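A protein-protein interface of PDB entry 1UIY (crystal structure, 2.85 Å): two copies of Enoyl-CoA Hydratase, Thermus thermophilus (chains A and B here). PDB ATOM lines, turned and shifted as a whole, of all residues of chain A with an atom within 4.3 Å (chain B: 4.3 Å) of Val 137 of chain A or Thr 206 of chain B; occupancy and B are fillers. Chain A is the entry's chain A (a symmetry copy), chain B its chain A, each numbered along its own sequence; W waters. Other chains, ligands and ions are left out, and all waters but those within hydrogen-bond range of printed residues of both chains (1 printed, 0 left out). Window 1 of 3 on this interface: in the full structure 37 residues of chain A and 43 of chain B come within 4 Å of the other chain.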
ATOM      1  N   GLU A 131      21.013  27.112 -17.395  1.00  0.00           N
ATOM      2  CA  GLU A 131      20.500  26.127 -18.340  1.00  0.00           C
ATOM      3  C   GLU A 131      19.670  26.692 -19.508  1.00  0.00           C
ATOM      4  O   GLU A 131      19.979  26.430 -20.674  1.00  0.00           O
ATOM      5  CB  GLU A 131      19.685  25.070 -17.592  1.00  0.00           C
ATOM      6  CG  GLU A 131      20.508  24.120 -16.727  1.00  0.00           C
ATOM      7  CD  GLU A 131      21.097  24.777 -15.476  1.00  0.00           C
ATOM      8  OE1 GLU A 131      21.848  24.093 -14.749  1.00  0.00           O
ATOM      9  OE2 GLU A 131      20.811  25.966 -15.216  1.00  0.00           O
ATOM     10  N   VAL A 132      18.628  27.464 -19.211  1.00  0.00           N
ATOM     11  CA  VAL A 132      17.791  28.006 -20.282  1.00  0.00           C
ATOM     12  C   VAL A 132      18.515  28.855 -21.326  1.00  0.00           C
ATOM     13  O   VAL A 132      18.143  28.847 -22.502  1.00  0.00           O
ATOM     14  CB  VAL A 132      16.626  28.848 -19.742  1.00  0.00           C
ATOM     15  CG1 VAL A 132      15.525  27.943 -19.268  1.00  0.00           C
ATOM     16  CG2 VAL A 132      17.116  29.769 -18.640  1.00  0.00           C
ATOM     17  N   PHE A 136      19.212  24.184 -21.920  1.00  0.00           N
ATOM     18  CA  PHE A 136      19.133  23.193 -20.859  1.00  0.00           C
ATOM     19  C   PHE A 136      18.023  23.551 -19.890  1.00  0.00           C
ATOM     20  O   PHE A 136      17.460  24.641 -19.952  1.00  0.00           O
ATOM     21  CB  PHE A 136      20.454  23.131 -20.096  1.00  0.00           C
ATOM     22  CG  PHE A 136      21.474  22.215 -20.709  1.00  0.00           C
ATOM     23  CD1 PHE A 136      22.834  22.492 -20.589  1.00  0.00           C
ATOM     24  CD2 PHE A 136      21.087  21.068 -21.383  1.00  0.00           C
ATOM     25  CE1 PHE A 136      23.791  21.639 -21.136  1.00  0.00           C
ATOM     26  CE2 PHE A 136      22.042  20.206 -21.934  1.00  0.00           C
ATOM     27  CZ  PHE A 136      23.392  20.494 -21.810  1.00  0.00           C
ATOM     28  N   VAL A 137      17.710  22.621 -18.994  1.00  0.00           N
ATOM     29  CA  VAL A 137      16.689  22.846 -17.982  1.00  0.00           C
ATOM     30  C   VAL A 137      17.270  22.499 -16.623  1.00  0.00           C
ATOM     31  O   VAL A 137      17.801  21.409 -16.431  1.00  0.00           O
ATOM     32  CB  VAL A 137      15.456  21.971 -18.207  1.00  0.00           C
ATOM     33  CG1 VAL A 137      14.542  22.063 -17.021  1.00  0.00           C
ATOM     34  CG2 VAL A 137      14.727  22.425 -19.430  1.00  0.00           C
ATOM     35  N   ALA A 138      17.180  23.420 -15.679  1.00  0.00           N
ATOM     36  CA  ALA A 138      17.691  23.148 -14.346  1.00  0.00           C
ATOM     37  C   ALA A 138      16.688  22.257 -13.608  1.00  0.00           C
ATOM     38  O   ALA A 138      16.383  22.481 -12.441  1.00  0.00           O
ATOM     39  CB  ALA A 138      17.905  24.456 -13.592  1.00  0.00           C
ATOM     40  N   ALA A 139      16.189  21.241 -14.302  1.00  0.00           N
ATOM     41  CA  ALA A 139      15.206  20.326 -13.736  1.00  0.00           C
ATOM     42  C   ALA A 139      15.582  19.756 -12.368  1.00  0.00           C
ATOM     43  O   ALA A 139      14.840  19.918 -11.397  1.00  0.00           O
ATOM     44  CB  ALA A 139      14.924  19.189 -14.724  1.00  0.00           C
ATOM     45  N   LEU A 158      15.332  30.980 -12.739  1.00  0.00           N
ATOM     46  CA  LEU A 158      15.344  29.987 -13.800  1.00  0.00           C
ATOM     47  C   LEU A 158      14.968  30.482 -15.177  1.00  0.00           C
ATOM     48  O   LEU A 158      15.396  29.887 -16.165  1.00  0.00           O
ATOM     49  CB  LEU A 158      14.464  28.790 -13.435  1.00  0.00           C
ATOM     50  CG  LEU A 158      14.832  28.051 -12.147  1.00  0.00           C
ATOM     51  CD1 LEU A 158      14.004  26.792 -12.048  1.00  0.00           C
ATOM     52  CD2 LEU A 158      16.311  27.711 -12.131  1.00  0.00           C
ATOM     53  N   LEU A 159      14.177  31.552 -15.260  1.00  0.00           N
ATOM     54  CA  LEU A 159      13.762  32.085 -16.566  1.00  0.00           C
ATOM     55  C   LEU A 159      14.768  33.066 -17.177  1.00  0.00           C
ATOM     56  O   LEU A 159      14.931  33.118 -18.398  1.00  0.00           O
ATOM     57  CB  LEU A 159      12.387  32.759 -16.475  1.00  0.00           C
ATOM     58  CG  LEU A 159      11.224  31.871 -16.030  1.00  0.00           C
ATOM     59  CD1 LEU A 159       9.927  32.620 -16.195  1.00  0.00           C
ATOM     60  CD2 LEU A 159      11.187  30.595 -16.847  1.00  0.00           C
ATOM     61  N   SER B 202      13.324  25.204 -23.210  1.00  0.00           N
ATOM     62  CA  SER B 202      13.760  25.237 -21.822  1.00  0.00           C
ATOM     63  C   SER B 202      12.841  26.042 -20.907  1.00  0.00           C
ATOM     64  O   SER B 202      12.647  25.684 -19.742  1.00  0.00           O
ATOM     65  CB  SER B 202      15.180  25.795 -21.733  1.00  0.00           C
ATOM     66  OG  SER B 202      16.089  24.943 -22.409  1.00  0.00           O
ATOM     67  N   LEU B 203      12.274  27.122 -21.437  1.00  0.00           N
ATOM     68  CA  LEU B 203      11.389  27.974 -20.654  1.00  0.00           C
ATOM     69  C   LEU B 203      10.088  27.272 -20.279  1.00  0.00           C
ATOM     70  O   LEU B 203       9.735  27.163 -19.105  1.00  0.00           O
ATOM     71  CB  LEU B 203      11.084  29.251 -21.431  1.00  0.00           C
ATOM     72  CG  LEU B 203      12.271  30.161 -21.752  1.00  0.00           C
ATOM     73  CD1 LEU B 203      11.765  31.349 -22.525  1.00  0.00           C
ATOM     74  CD2 LEU B 203      12.962  30.626 -20.473  1.00  0.00           C
ATOM     75  N   ARG B 204       9.376  26.805 -21.289  1.00  0.00           N
ATOM     76  CA  ARG B 204       8.119  26.112 -21.083  1.00  0.00           C
ATOM     77  C   ARG B 204       8.295  25.027 -20.022  1.00  0.00           C
ATOM     78  O   ARG B 204       7.636  25.036 -18.981  1.00  0.00           O
ATOM     79  CB  ARG B 204       7.675  25.474 -22.401  1.00  0.00           C
ATOM     80  CG  ARG B 204       6.222  25.032 -22.469  1.00  0.00           C
ATOM     81  CD  ARG B 204       5.930  24.566 -23.878  1.00  0.00           C
ATOM     82  NE  ARG B 204       6.556  25.467 -24.850  1.00  0.00           N
ATOM     83  CZ  ARG B 204       7.109  25.079 -25.999  1.00  0.00           C
ATOM     84  NH1 ARG B 204       7.117  23.795 -26.343  1.00  0.00           N
ATOM     85  NH2 ARG B 204       7.679  25.976 -26.797  1.00  0.00           N
ATOM     86  N   LEU B 205       9.197  24.095 -20.301  1.00  0.00           N
ATOM     87  CA  LEU B 205       9.455  22.981 -19.410  1.00  0.00           C
ATOM     88  C   LEU B 205       9.789  23.414 -17.977  1.00  0.00           C
ATOM     89  O   LEU B 205       9.283  22.834 -17.010  1.00  0.00           O
ATOM     90  CB  LEU B 205      10.578  22.128 -20.004  1.00  0.00           C
ATOM     91  CG  LEU B 205      10.805  20.751 -19.389  1.00  0.00           C
ATOM     92  CD1 LEU B 205       9.488  19.992 -19.279  1.00  0.00           C
ATOM     93  CD2 LEU B 205      11.802  20.006 -20.248  1.00  0.00           C
ATOM     94  N   THR B 206      10.649  24.419 -17.846  1.00  0.00           N
ATOM     95  CA  THR B 206      11.023  24.933 -16.536  1.00  0.00           C
ATOM     96  C   THR B 206       9.729  25.322 -15.826  1.00  0.00           C
ATOM     97  O   THR B 206       9.551  25.086 -14.631  1.00  0.00           O
ATOM     98  CB  THR B 206      11.919  26.183 -16.664  1.00  0.00           C
ATOM     99  OG1 THR B 206      13.180  25.815 -17.235  1.00  0.00           O
ATOM    100  CG2 THR B 206      12.152  26.823 -15.305  1.00  0.00           C
ATOM    101  N   LYS B 207       8.822  25.923 -16.583  1.00  0.00           N
ATOM    102  CA  LYS B 207       7.546  26.336 -16.040  1.00  0.00           C
ATOM    103  C   LYS B 207       6.717  25.100 -15.689  1.00  0.00           C
ATOM    104  O   LYS B 207       6.150  25.003 -14.589  1.00  0.00           O
ATOM    105  CB  LYS B 207       6.824  27.234 -17.054  1.00  0.00           C
ATOM    106  CG  LYS B 207       7.369  28.666 -17.064  1.00  0.00           C
ATOM    107  CD  LYS B 207       7.066  29.431 -18.351  1.00  0.00           C
ATOM    108  CE  LYS B 207       5.583  29.551 -18.626  1.00  0.00           C
ATOM    109  NZ  LYS B 207       4.875  30.265 -17.551  1.00  0.00           N
ATOM    110  N   GLU B 208       6.666  24.151 -16.618  1.00  0.00           N
ATOM    111  CA  GLU B 208       5.919  22.920 -16.402  1.00  0.00           C
ATOM    112  C   GLU B 208       6.362  22.295 -15.077  1.00  0.00           C
ATOM    113  O   GLU B 208       5.544  21.930 -14.238  1.00  0.00           O
ATOM    114  CB  GLU B 208       6.181  21.944 -17.552  1.00  0.00           C
ATOM    115  CG  GLU B 208       5.330  20.688 -17.496  1.00  0.00           C
ATOM    116  CD  GLU B 208       3.914  20.929 -17.976  1.00  0.00           C
ATOM    117  OE1 GLU B 208       3.304  21.962 -17.588  1.00  0.00           O
ATOM    118  OE2 GLU B 208       3.409  20.073 -18.743  1.00  0.00           O
ATOM    119  N   LEU B 209       7.673  22.186 -14.902  1.00  0.00           N
ATOM    120  CA  LEU B 209       8.239  21.621 -13.690  1.00  0.00           C
ATOM    121  C   LEU B 209       7.829  22.365 -12.426  1.00  0.00           C
ATOM    122  O   LEU B 209       7.389  21.753 -11.449  1.00  0.00           O
ATOM    123  CB  LEU B 209       9.761  21.612 -13.772  1.00  0.00           C
ATOM    124  CG  LEU B 209      10.438  20.496 -14.560  1.00  0.00           C
ATOM    125  CD1 LEU B 209      11.943  20.695 -14.460  1.00  0.00           C
ATOM    126  CD2 LEU B 209      10.050  19.127 -14.004  1.00  0.00           C
ATOM    127  N   LEU B 210       7.985  23.682 -12.436  1.00  0.00           N
ATOM    128  CA  LEU B 210       7.648  24.479 -11.258  1.00  0.00           C
ATOM    129  C   LEU B 210       6.186  24.365 -10.868  1.00  0.00           C
ATOM    130  O   LEU B 210       5.802  24.717  -9.761  1.00  0.00           O
ATOM    131  CB  LEU B 210       8.003  25.946 -11.486  1.00  0.00           C
ATOM    132  CG  LEU B 210       9.480  26.205 -11.756  1.00  0.00           C
ATOM    133  CD1 LEU B 210       9.699  27.695 -11.968  1.00  0.00           C
ATOM    134  CD2 LEU B 210      10.307  25.688 -10.590  1.00  0.00           C
ATOM    135  N   ASN B 229      15.229  16.224 -17.587  1.00  0.00           N
ATOM    136  CA  ASN B 229      16.631  16.481 -17.858  1.00  0.00           C
ATOM    137  C   ASN B 229      17.017  15.634 -19.063  1.00  0.00           C
ATOM    138  O   ASN B 229      17.833  16.036 -19.891  1.00  0.00           O
ATOM    139  CB  ASN B 229      17.468  16.074 -16.647  1.00  0.00           C
ATOM    140  CG  ASN B 229      18.910  16.511 -16.764  1.00  0.00           C
ATOM    141  OD1 ASN B 229      19.233  17.671 -16.518  1.00  0.00           O
ATOM    142  ND2 ASN B 229      19.787  15.587 -17.150  1.00  0.00           N
ATOM    143  N   VAL B 232      14.867  16.837 -22.597  1.00  0.00           N
ATOM    144  CA  VAL B 232      15.439  18.101 -23.049  1.00  0.00           C
ATOM    145  C   VAL B 232      16.725  17.916 -23.882  1.00  0.00           C
ATOM    146  O   VAL B 232      17.053  18.740 -24.740  1.00  0.00           O
ATOM    147  CB  VAL B 232      15.724  19.020 -21.808  1.00  0.00           C
ATOM    148  CG1 VAL B 232      17.033  18.630 -21.150  1.00  0.00           C
ATOM    149  CG2 VAL B 232      15.726  20.478 -22.203  1.00  0.00           C
HETATM  150  O   HOH W   1      15.921  25.734 -16.204  1.00  0.00           O
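CG1 of Val 132 of chain A touches CB of Ser 202 of chain B (3.3 Å). Val 132 of chain A touches Leu 203 of chain B. CG1 of Val 132 of chain A touches OG1 of Thr 206 of chain B (3.8 Å). CA of Ser 202 of chain B touches CG2 of Val 137 of chain A (3.8 Å). Val 137 of chain A touches Leu 205 of chain B. Thr 206 of chain B touches Val 137 of chain A (OG1 to CG1, 3.997 Å). CG1 of Val 137 of chain A touches CD1 of Leu 209 of chain B, 3.9 Å away. CG2 of Val 137 of chain A touches CG2 of Val 232 of chain B, at 3.5 Å. Leu 209 of chain B touches Ala 139 of chain A. Leu 158 of chain A touches Thr 206 of chain B.
The backbone carbonyl oxygen of Ser 202 of chain B is in hydrogen-bond range of the side-chain hydroxyl of Thr 206 of chain B, at 2.6 Å. The backbone carbonyl oxygen (O) of Glu 131 of chain A lies within hydrogen-bond range of the backbone NH (N) of Phe 136 of chain A (2.7 Å).
Hydrophobic or aromatic side chains of chain B within 4 Å of the printed part of chain A: Leu 203, Leu 205, Leu 209 and Val 232. Of the 8 printed residues of chain A, 6 touch a printed residue of chain B. Printed residues of chain A that touch a printed residue of chain B: Val 132, Phe 136, Val 137, Ala 139, Leu 158 and Leu 159. Hydrophobic or aromatic side chains of chain A within 4 Å of the printed part of chain B: Val 132, Val 137, Ala 139 and Leu 158. Along chain A the printed residues that touch a printed residue of chain B span positions 132 to 159. Among the printed residues, 12 pairs touch across the chains. Among the printed residues, no Asp or Glu carboxylate lies within 4 Å of a Lys or Arg side-chain nitrogen of the other chain.
No position is printed for both chains. Of the 12 pairs that touch across the chains among the printed residues, none has its exchanged pair printed and touching as well.
Of the printed residues of chain B, Val 137 of chain A touches Ser 202, Leu 205, Thr 206, Leu 209 and Val 232. Of the printed residues of chain A, Thr 206 of chain B touches Val 132, Val 137 and Leu 158. Printed residues of chain A within 4 Å of Leu 205 of chain B: Val 137. Of the printed residues of chain B, Phe 136 of chain A touches Ser 202 (2.8 Å). Ala 138 of chain A touches none of the printed residues of chain B. Leu 210 of chain B touches none of the printed residues of chain A. The nearest printed residue of chain A that does not touch Thr 206 of chain B is Leu 159 of chain A (4.2 Å). The nearest printed residue of chain A that does not touch Leu 209 of chain B is Ala 138 of chain A (5.1 Å).
O of Phe 136 of chain A lies within hydrogen-bond range of OG of Ser 202 of chain B, 2.8 Å away.
Water W1 bridges N of Ala 138 of chain A (2.7 Å) and OG1 of Thr 206 of chain B (2.9 Å).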
